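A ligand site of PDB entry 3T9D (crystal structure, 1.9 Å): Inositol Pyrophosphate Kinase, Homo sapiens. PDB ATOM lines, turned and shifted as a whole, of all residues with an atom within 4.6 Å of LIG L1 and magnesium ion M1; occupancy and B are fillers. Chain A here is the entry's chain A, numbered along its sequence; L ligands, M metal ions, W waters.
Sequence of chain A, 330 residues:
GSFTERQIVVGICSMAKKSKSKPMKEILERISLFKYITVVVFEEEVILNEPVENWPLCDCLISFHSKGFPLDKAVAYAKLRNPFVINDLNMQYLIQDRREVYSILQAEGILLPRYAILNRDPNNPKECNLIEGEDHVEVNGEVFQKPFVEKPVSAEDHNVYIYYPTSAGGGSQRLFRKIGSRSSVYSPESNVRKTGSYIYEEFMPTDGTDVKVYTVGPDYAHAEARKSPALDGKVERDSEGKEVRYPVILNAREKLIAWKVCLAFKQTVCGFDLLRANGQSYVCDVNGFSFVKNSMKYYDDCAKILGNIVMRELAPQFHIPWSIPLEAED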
ATOM      1  N   LYS A  17      31.101  10.982 -14.477  1.00  0.00           N
ATOM      2  CA  LYS A  17      30.115  10.103 -15.132  1.00  0.00           C
ATOM      3  C   LYS A  17      30.341  10.015 -16.650  1.00  0.00           C
ATOM      4  O   LYS A  17      30.163   8.950 -17.281  1.00  0.00           O
ATOM      5  CB  LYS A  17      28.709  10.629 -14.839  1.00  0.00           C
ATOM      6  CG  LYS A  17      27.551   9.758 -15.325  1.00  0.00           C
ATOM      7  CD  LYS A  17      26.236  10.358 -14.844  1.00  0.00           C
ATOM      8  CE  LYS A  17      25.041   9.650 -15.425  1.00  0.00           C
ATOM      9  NZ  LYS A  17      23.781  10.208 -14.850  1.00  0.00           N
ATOM     10  N   LYS A  18      30.751  11.141 -17.228  1.00  0.00           N
ATOM     11  CA  LYS A  18      31.020  11.208 -18.661  1.00  0.00           C
ATOM     12  C   LYS A  18      32.488  10.867 -19.006  1.00  0.00           C
ATOM     13  O   LYS A  18      32.735  10.053 -19.910  1.00  0.00           O
ATOM     14  CB  LYS A  18      30.635  12.573 -19.245  1.00  0.00           C
ATOM     15  CG  LYS A  18      29.196  13.053 -18.894  1.00  0.00           C
ATOM     16  CD  LYS A  18      28.112  12.179 -19.544  1.00  0.00           C
ATOM     17  CE  LYS A  18      26.694  12.696 -19.223  1.00  0.00           C
ATOM     18  NZ  LYS A  18      25.649  11.696 -19.596  1.00  0.00           N
ATOM     19  N   SER A  66      27.042  18.615 -18.586  1.00  0.00           N
ATOM     20  CA  SER A  66      25.977  17.680 -18.247  1.00  0.00           C
ATOM     21  C   SER A  66      25.496  18.027 -16.836  1.00  0.00           C
ATOM     22  O   SER A  66      26.026  18.953 -16.212  1.00  0.00           O
ATOM     23  CB  SER A  66      26.451  16.232 -18.339  1.00  0.00           C
ATOM     24  OG  SER A  66      27.496  15.950 -17.438  1.00  0.00           O
ATOM     25  N   HIS A 158      13.332  15.860 -19.188  1.00  0.00           N
ATOM     26  CA  HIS A 158      12.959  14.863 -20.205  1.00  0.00           C
ATOM     27  C   HIS A 158      11.497  14.375 -20.094  1.00  0.00           C
ATOM     28  O   HIS A 158      11.108  13.384 -20.721  1.00  0.00           O
ATOM     29  CB  HIS A 158      13.952  13.685 -20.165  1.00  0.00           C
ATOM     30  CG  HIS A 158      15.371  14.133 -20.362  1.00  0.00           C
ATOM     31  ND1 HIS A 158      15.791  14.747 -21.526  1.00  0.00           N
ATOM     32  CD2 HIS A 158      16.434  14.159 -19.526  1.00  0.00           C
ATOM     33  CE1 HIS A 158      17.057  15.092 -21.408  1.00  0.00           C
ATOM     34  NE2 HIS A 158      17.477  14.750 -20.211  1.00  0.00           N
ATOM     35  N   ARG A 177      13.364   9.905 -18.819  1.00  0.00           N
ATOM     36  CA  ARG A 177      14.653   9.196 -18.845  1.00  0.00           C
ATOM     37  C   ARG A 177      14.407   7.744 -18.483  1.00  0.00           C
ATOM     38  O   ARG A 177      13.705   7.472 -17.500  1.00  0.00           O
ATOM     39  CB  ARG A 177      15.650   9.783 -17.824  1.00  0.00           C
ATOM     40  CG  ARG A 177      16.700  10.736 -18.387  1.00  0.00           C
ATOM     41  CD  ARG A 177      17.786  10.034 -19.230  1.00  0.00           C
ATOM     42  NE  ARG A 177      18.561  11.002 -20.004  1.00  0.00           N
ATOM     43  CZ  ARG A 177      18.229  11.437 -21.215  1.00  0.00           C
ATOM     44  NH1 ARG A 177      17.138  10.961 -21.811  1.00  0.00           N
ATOM     45  NH2 ARG A 177      18.983  12.323 -21.849  1.00  0.00           N
ATOM     46  N   LYS A 178      14.947   6.821 -19.273  1.00  0.00           N
ATOM     47  CA  LYS A 178      14.713   5.386 -19.075  1.00  0.00           C
ATOM     48  C   LYS A 178      14.921   4.968 -17.628  1.00  0.00           C
ATOM     49  O   LYS A 178      15.914   5.358 -16.991  1.00  0.00           O
ATOM     50  CB  LYS A 178      15.611   4.542 -19.981  1.00  0.00           C
ATOM     51  CG  LYS A 178      15.040   4.338 -21.364  1.00  0.00           C
ATOM     52  CD  LYS A 178      16.023   3.599 -22.291  1.00  0.00           C
ATOM     53  CE  LYS A 178      17.023   4.572 -22.932  1.00  0.00           C
ATOM     54  NZ  LYS A 178      18.123   3.860 -23.658  1.00  0.00           N
ATOM     55  N   LYS A 212      18.844   8.679 -34.432  1.00  0.00           N
ATOM     56  CA  LYS A 212      19.824   9.430 -33.632  1.00  0.00           C
ATOM     57  C   LYS A 212      21.054   9.617 -34.503  1.00  0.00           C
ATOM     58  O   LYS A 212      21.558   8.651 -35.108  1.00  0.00           O
ATOM     59  CB  LYS A 212      20.200   8.685 -32.357  1.00  0.00           C
ATOM     60  CG  LYS A 212      19.008   8.226 -31.526  1.00  0.00           C
ATOM     61  CD  LYS A 212      18.444   9.313 -30.665  1.00  0.00           C
ATOM     62  CE  LYS A 212      19.243   9.482 -29.373  1.00  0.00           C
ATOM     63  NZ  LYS A 212      18.834  10.715 -28.624  1.00  0.00           N
ATOM     64  N   TYR A 214      25.032  11.286 -34.804  1.00  0.00           N
ATOM     65  CA  TYR A 214      26.187  11.624 -33.992  1.00  0.00           C
ATOM     66  C   TYR A 214      27.256  12.168 -34.919  1.00  0.00           C
ATOM     67  O   TYR A 214      27.785  11.422 -35.746  1.00  0.00           O
ATOM     68  CB  TYR A 214      26.718  10.371 -33.297  1.00  0.00           C
ATOM     69  CG  TYR A 214      25.714   9.715 -32.361  1.00  0.00           C
ATOM     70  CD1 TYR A 214      24.797   8.794 -32.843  1.00  0.00           C
ATOM     71  CD2 TYR A 214      25.708  10.025 -30.997  1.00  0.00           C
ATOM     72  CE1 TYR A 214      23.875   8.181 -31.975  1.00  0.00           C
ATOM     73  CE2 TYR A 214      24.790   9.419 -30.122  1.00  0.00           C
ATOM     74  CZ  TYR A 214      23.887   8.495 -30.624  1.00  0.00           C
ATOM     75  OH  TYR A 214      22.975   7.893 -29.770  1.00  0.00           O
ATOM     76  N   ARG A 237      15.525  -4.592 -25.435  1.00  0.00           N
ATOM     77  CA  ARG A 237      16.901  -4.820 -25.014  1.00  0.00           C
ATOM     78  C   ARG A 237      17.454  -6.100 -25.611  1.00  0.00           C
ATOM     79  O   ARG A 237      16.716  -7.007 -25.857  1.00  0.00           O
ATOM     80  CB  ARG A 237      17.011  -4.840 -23.492  1.00  0.00           C
ATOM     81  CG  ARG A 237      16.667  -3.498 -22.874  1.00  0.00           C
ATOM     82  CD  ARG A 237      17.371  -3.191 -21.594  1.00  0.00           C
ATOM     83  NE  ARG A 237      17.020  -1.906 -21.050  1.00  0.00           N
ATOM     84  CZ  ARG A 237      17.804  -0.850 -21.019  1.00  0.00           C
ATOM     85  NH1 ARG A 237      19.017  -0.924 -21.507  1.00  0.00           N
ATOM     86  NH2 ARG A 237      17.380   0.286 -20.491  1.00  0.00           N
ATOM     87  N   GLU A 243      20.135  -1.415 -25.334  1.00  0.00           N
ATOM     88  CA  GLU A 243      18.969  -1.075 -26.151  1.00  0.00           C
ATOM     89  C   GLU A 243      19.214  -1.489 -27.606  1.00  0.00           C
ATOM     90  O   GLU A 243      20.298  -1.276 -28.136  1.00  0.00           O
ATOM     91  CB  GLU A 243      18.591   0.415 -26.060  1.00  0.00           C
ATOM     92  CG  GLU A 243      17.268   0.753 -26.777  1.00  0.00           C
ATOM     93  CD  GLU A 243      16.811   2.188 -26.610  1.00  0.00           C
ATOM     94  OE1 GLU A 243      17.548   3.008 -26.044  1.00  0.00           O
ATOM     95  OE2 GLU A 243      15.679   2.496 -27.058  1.00  0.00           O
ATOM     96  N   ARG A 245      19.333  -1.280 -31.436  1.00  0.00           N
ATOM     97  CA  ARG A 245      19.513  -0.176 -32.375  1.00  0.00           C
ATOM     98  C   ARG A 245      19.417  -0.729 -33.800  1.00  0.00           C
ATOM     99  O   ARG A 245      19.820  -1.855 -34.053  1.00  0.00           O
ATOM    100  CB  ARG A 245      20.850   0.554 -32.117  1.00  0.00           C
ATOM    101  CG  ARG A 245      20.914   1.391 -30.795  1.00  0.00           C
ATOM    102  CD  ARG A 245      20.171   2.740 -30.947  1.00  0.00           C
ATOM    103  NE  ARG A 245      19.938   3.475 -29.694  1.00  0.00           N
ATOM    104  CZ  ARG A 245      20.527   4.631 -29.375  1.00  0.00           C
ATOM    105  NH1 ARG A 245      21.425   5.191 -30.184  1.00  0.00           N
ATOM    106  NH2 ARG A 245      20.227   5.229 -28.224  1.00  0.00           N
ATOM    107  N   ASN A 287      21.294  17.740 -28.828  1.00  0.00           N
ATOM    108  CA  ASN A 287      21.817  17.462 -27.484  1.00  0.00           C
ATOM    109  C   ASN A 287      23.244  17.917 -27.204  1.00  0.00           C
ATOM    110  O   ASN A 287      23.662  17.978 -26.045  1.00  0.00           O
ATOM    111  CB  ASN A 287      21.684  15.969 -27.158  1.00  0.00           C
ATOM    112  CG  ASN A 287      20.245  15.525 -27.141  1.00  0.00           C
ATOM    113  OD1 ASN A 287      19.900  14.474 -27.695  1.00  0.00           O
ATOM    114  ND2 ASN A 287      19.387  16.318 -26.512  1.00  0.00           N
ATOM    115  N   PHE A 289      27.275  17.431 -27.068  1.00  0.00           N
ATOM    116  CA  PHE A 289      28.277  16.364 -26.943  1.00  0.00           C
ATOM    117  C   PHE A 289      27.687  15.026 -26.586  1.00  0.00           C
ATOM    118  O   PHE A 289      27.037  14.866 -25.543  1.00  0.00           O
ATOM    119  CB  PHE A 289      29.356  16.726 -25.925  1.00  0.00           C
ATOM    120  CG  PHE A 289      30.636  15.942 -26.110  1.00  0.00           C
ATOM    121  CD1 PHE A 289      30.737  14.626 -25.663  1.00  0.00           C
ATOM    122  CD2 PHE A 289      31.723  16.536 -26.734  1.00  0.00           C
ATOM    123  CE1 PHE A 289      31.935  13.904 -25.832  1.00  0.00           C
ATOM    124  CE2 PHE A 289      32.911  15.831 -26.912  1.00  0.00           C
ATOM    125  CZ  PHE A 289      33.019  14.509 -26.464  1.00  0.00           C
ATOM    126  N   SER A 290      27.921  14.052 -27.457  1.00  0.00           N
ATOM    127  CA  SER A 290      27.381  12.720 -27.316  1.00  0.00           C
ATOM    128  C   SER A 290      28.184  11.744 -28.185  1.00  0.00           C
ATOM    129  O   SER A 290      28.445  12.034 -29.352  1.00  0.00           O
ATOM    130  CB  SER A 290      25.893  12.678 -27.698  1.00  0.00           C
ATOM    131  OG  SER A 290      25.384  11.375 -27.444  1.00  0.00           O
ATOM    132  N   LYS A 293      27.504   4.573 -28.548  1.00  0.00           N
ATOM    133  CA  LYS A 293      27.848   3.484 -27.627  1.00  0.00           C
ATOM    134  C   LYS A 293      27.895   2.147 -28.365  1.00  0.00           C
ATOM    135  O   LYS A 293      27.053   1.861 -29.217  1.00  0.00           O
ATOM    136  CB  LYS A 293      26.825   3.407 -26.475  1.00  0.00           C
ATOM    137  CG  LYS A 293      26.881   4.569 -25.464  1.00  0.00           C
ATOM    138  CD  LYS A 293      26.045   5.756 -25.911  1.00  0.00           C
ATOM    139  CE  LYS A 293      26.112   6.927 -24.928  1.00  0.00           C
ATOM    140  NZ  LYS A 293      25.570   8.181 -25.546  1.00  0.00           N
HETATM  141  C1  LIG L   1      21.472   9.826 -23.371  1.00  0.00           C
HETATM  142  C2  LIG L   1      22.406  10.622 -22.458  1.00  0.00           C
HETATM  143  C3  LIG L   1      21.941  10.421 -21.003  1.00  0.00           C
HETATM  144  C4  LIG L   1      21.993   8.954 -20.584  1.00  0.00           C
HETATM  145  C5  LIG L   1      21.189   8.084 -21.558  1.00  0.00           C
HETATM  146  C6  LIG L   1      21.531   8.336 -23.035  1.00  0.00           C
HETATM  147  O1  LIG L   1      21.832  10.021 -24.749  1.00  0.00           O
HETATM  148  O2  LIG L   1      23.746  10.167 -22.620  1.00  0.00           O
HETATM  149  O3  LIG L   1      22.754  11.193 -20.092  1.00  0.00           O
HETATM  150  O4  LIG L   1      21.350   8.862 -19.332  1.00  0.00           O
HETATM  151  O5  LIG L   1      21.428   6.705 -21.257  1.00  0.00           O
HETATM  152  O6  LIG L   1      20.560   7.633 -23.809  1.00  0.00           O
HETATM  153  O7  LIG L   1      19.413  10.794 -25.415  1.00  0.00           O
HETATM  154  O8  LIG L   1      25.260  12.234 -22.259  1.00  0.00           O
HETATM  155  O9  LIG L   1      20.875  11.844 -18.484  1.00  0.00           O
HETATM  156  O10 LIG L   1      22.549   9.953 -17.328  1.00  0.00           O
HETATM  157  O11 LIG L   1      19.032   6.553 -20.318  1.00  0.00           O
HETATM  158  O12 LIG L   1      19.768   5.466 -24.909  1.00  0.00           O
HETATM  159  O13 LIG L   1      21.307  12.514 -25.049  1.00  0.00           O
HETATM  160  O14 LIG L   1      24.341  11.800 -24.616  1.00  0.00           O
HETATM  161  O15 LIG L   1      21.427  13.359 -20.539  1.00  0.00           O
HETATM  162  O16 LIG L   1      23.527   7.786 -18.358  1.00  0.00           O
HETATM  163  O17 LIG L   1      20.985   5.329 -19.210  1.00  0.00           O
HETATM  164  O18 LIG L   1      22.220   5.607 -24.090  1.00  0.00           O
HETATM  165  O19 LIG L   1      21.367  10.933 -27.113  1.00  0.00           O
HETATM  166  O20 LIG L   1      26.088  10.199 -23.641  1.00  0.00           O
HETATM  167  O21 LIG L   1      23.128  13.230 -18.572  1.00  0.00           O
HETATM  168  O22 LIG L   1      21.270   7.708 -17.042  1.00  0.00           O
HETATM  169  O23 LIG L   1      20.106   4.615 -21.485  1.00  0.00           O
HETATM  170  O24 LIG L   1      21.455   6.986 -26.120  1.00  0.00           O
HETATM  171  O25 LIG L   1      19.442   2.728 -19.831  1.00  0.00           O
HETATM  172  O26 LIG L   1      19.816   2.197 -22.312  1.00  0.00           O
HETATM  173  O27 LIG L   1      21.858   2.847 -20.809  1.00  0.00           O
HETATM  174  P1  LIG L   1      20.994  11.062 -25.669  1.00  0.00           P
HETATM  175  P2  LIG L   1      24.933  11.058 -23.315  1.00  0.00           P
HETATM  176  P3  LIG L   1      22.102  12.471 -19.354  1.00  0.00           P
HETATM  177  P4  LIG L   1      22.142   8.511 -17.951  1.00  0.00           P
HETATM  178  P5  LIG L   1      20.324   5.830 -20.435  1.00  0.00           P
HETATM  179  P6  LIG L   1      21.031   6.466 -24.793  1.00  0.00           P
HETATM  180  P7  LIG L   1      20.411   3.078 -21.081  1.00  0.00           P
HETATM  181  P1  LG2 L   2      16.850  13.060 -25.342  1.00  0.00           P
HETATM  182  O1  LG2 L   2      17.092  12.664 -26.856  1.00  0.00           O
HETATM  183  O2  LG2 L   2      17.239  12.079 -24.340  1.00  0.00           O
HETATM  184  O3  LG2 L   2      17.613  14.509 -25.101  1.00  0.00           O
HETATM  185  P2  LG2 L   2      14.486  14.773 -24.944  1.00  0.00           P
HETATM  186  O4  LG2 L   2      13.881  14.830 -23.601  1.00  0.00           O
HETATM  187  O5  LG2 L   2      15.390  15.903 -25.328  1.00  0.00           O
HETATM  188  N1  LG2 L   2      15.152  13.327 -25.198  1.00  0.00           N
HETATM  189  P3  LG2 L   2      12.917  14.741 -27.428  1.00  0.00           P
HETATM  190  O6  LG2 L   2      12.624  16.080 -27.994  1.00  0.00           O
HETATM  191  O7  LG2 L   2      13.964  13.927 -28.067  1.00  0.00           O
HETATM  192  O8  LG2 L   2      13.128  14.831 -25.842  1.00  0.00           O
HETATM  193  O9  LG2 L   2      11.572  13.922 -27.416  1.00  0.00           O
HETATM  194  C1  LG2 L   2      11.577  12.563 -26.981  1.00  0.00           C
HETATM  195  C2  LG2 L   2      10.959  11.620 -28.032  1.00  0.00           C
HETATM  196  O10 LG2 L   2       9.625  12.050 -28.295  1.00  0.00           O
HETATM  197  C3  LG2 L   2      11.686  11.710 -29.355  1.00  0.00           C
HETATM  198  O11 LG2 L   2      12.759  10.792 -29.356  1.00  0.00           O
HETATM  199  C4  LG2 L   2      10.608  11.275 -30.324  1.00  0.00           C
HETATM  200  O12 LG2 L   2      10.441   9.840 -30.319  1.00  0.00           O
HETATM  201  C5  LG2 L   2       9.363  11.893 -29.709  1.00  0.00           C
HETATM  202  N2  LG2 L   2       9.051  13.220 -30.298  1.00  0.00           N
HETATM  203  C6  LG2 L   2       9.520  14.513 -29.836  1.00  0.00           C
HETATM  204  N3  LG2 L   2       8.861  15.427 -30.737  1.00  0.00           N
HETATM  205  C7  LG2 L   2       8.125  14.729 -31.611  1.00  0.00           C
HETATM  206  C8  LG2 L   2       7.341  15.148 -32.613  1.00  0.00           C
HETATM  207  N4  LG2 L   2       7.260  16.469 -32.831  1.00  0.00           N
HETATM  208  N5  LG2 L   2       6.666  14.288 -33.377  1.00  0.00           N
HETATM  209  C9  LG2 L   2       6.785  12.920 -33.152  1.00  0.00           C
HETATM  210  N6  LG2 L   2       7.596  12.498 -32.090  1.00  0.00           N
HETATM  211  C10 LG2 L   2       8.237  13.411 -31.341  1.00  0.00           C
HETATM  212 MG    MG M   1      20.305   5.869 -17.263  1.00  0.00          MG
HETATM  213 MG    MG M   2      23.740  16.049 -22.696  1.00  0.00          MG
HETATM  214  O   HOH W   1      20.034  14.312 -23.697  1.00  0.00           O
HETATM  215  O   HOH W   2      16.353   7.817 -21.552  1.00  0.00           O
HETATM  216  O   HOH W   3      25.834   9.138 -18.731  1.00  0.00           O
HETATM  217  O   HOH W   4      24.548  15.250 -24.540  1.00  0.00           O
HETATM  218  O   HOH W   5      22.201  12.797 -28.665  1.00  0.00           O
HETATM  219  O   HOH W   6      18.944  13.175 -17.347  1.00  0.00           O
HETATM  220  O   HOH W   7      22.932  15.707 -18.271  1.00  0.00           O
HETATM  221  O   HOH W   8      28.347  10.394 -24.717  1.00  0.00           O
HETATM  222  O   HOH W   9      19.575   6.083 -15.217  1.00  0.00           O
HETATM  223  O   HOH W  10      20.132  15.648 -20.153  1.00  0.00           O
HETATM  224  O   HOH W  11      27.130  14.002 -22.839  1.00  0.00           O
HETATM  225  O   HOH W  12      23.465  14.161 -21.762  1.00  0.00           O
HETATM  226  O   HOH W  13      19.440   3.723 -17.267  1.00  0.00           O
HETATM  227  O   HOH W  14      22.164   4.869 -16.488  1.00  0.00           O
HETATM  228  O   HOH W  15      18.197   6.581 -17.939  1.00  0.00           O
HETATM  229  O   HOH W  16      22.973   8.727 -27.278  1.00  0.00           O
HETATM  230  O   HOH W  17      24.273  13.132 -16.223  1.00  0.00           O
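Magnesium ion M1 is bound by an oxygen (O22) of LIG L1 (2.1 Å), an oxygen (O17) of LIG L1 (2.1 Å), water W9 (2.2 Å), water W14 (2.2 Å), water W13 (2.3 Å) and water W15 (2.3 Å).
No residue comes within 4 Å of magnesium ion M1.
OE1 of Glu 243 touches O12 of LIG L1, at 3.5 Å. Asn 287 touches LIG L1 (OD1 to O13, 3.6 Å). Of the 15 residues printed, 11 come within 4 Å of LIG L1. The nearest printed residue that does not touch LIG L1 is Tyr 214 (4.1 Å).
Water W15 bridges O11 of LIG L1 and O of Lys 178. Water W6 bridges O9 of LIG L1 (2.6 Å) and NE of Arg 177 (3.5 Å). Water W17 bridges O21 of LIG L1 (2.6 Å) and NZ of Lys 17 (3.3 Å). Water W10 lies within hydrogen-bond range of O15 of LIG L1 and NE2 of His 158. Water W3 bridges an oxygen (O16) of LIG L1 (2.7 Å) and the side-chain amino group of Lys 18 (2.7 Å). Water W2 lies within hydrogen-bond range of the backbone NH (N) of Lys 178, an oxygen (O11) of LIG L1 and the guanidinium group (NH1) of Arg 177.
NZ of Lys 178 lies within salt-bridge range of O12 of LIG L1. O8 of LIG L1 is in salt-bridge range of NZ of Lys 18, at 2.7 Å. O10 of LIG L1 lies within salt-bridge range of NZ of Lys 17, 2.8 Å away. The side-chain amino group (NZ) of Lys 293 lies within salt-bridge range of an oxygen (O20) of LIG L1. An oxygen (O9) of LIG L1 is in salt-bridge range of the guanidinium group (NE) of Arg 177 (2.9 Å). NZ of Lys 212 lies within salt-bridge range of O19 of LIG L1 (3.0 Å). NH2 of Arg 245 is in salt-bridge range of O24 of LIG L1, 3.0 Å away. The side-chain hydroxyl of Ser 290 lies within hydrogen-bond range of an oxygen (O14) of LIG L1, at 3.0 Å. The guanidinium group of Arg 237 is in salt-bridge range of an oxygen (O25) of LIG L1 (3.3 Å). O2 of LG2 L2 is in salt-bridge range of NH1 of Arg 177 (2.8 Å). The side-chain amino group of Lys 212 sits close to an oxygen (O1) of LG2 L2. An oxygen (O4) of LG2 L2 is in hydrogen-bond range of a ring nitrogen (ND1) of His 158.
NZ of Lys 178 lies within salt-bridge range of OE1 of Glu 243, 2.6 Å away. A ring nitrogen (NE2) of His 158 lies within hydrogen-bond range of the guanidinium group of Arg 177 (3.3 Å). The side-chain hydroxyl (OH) of Tyr 214 lies within hydrogen-bond range of the guanidinium group (NH1) of Arg 245 (3.1 Å).
O2 of LG2 L2 sits close to O7 of LIG L1 (2.7 Å).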
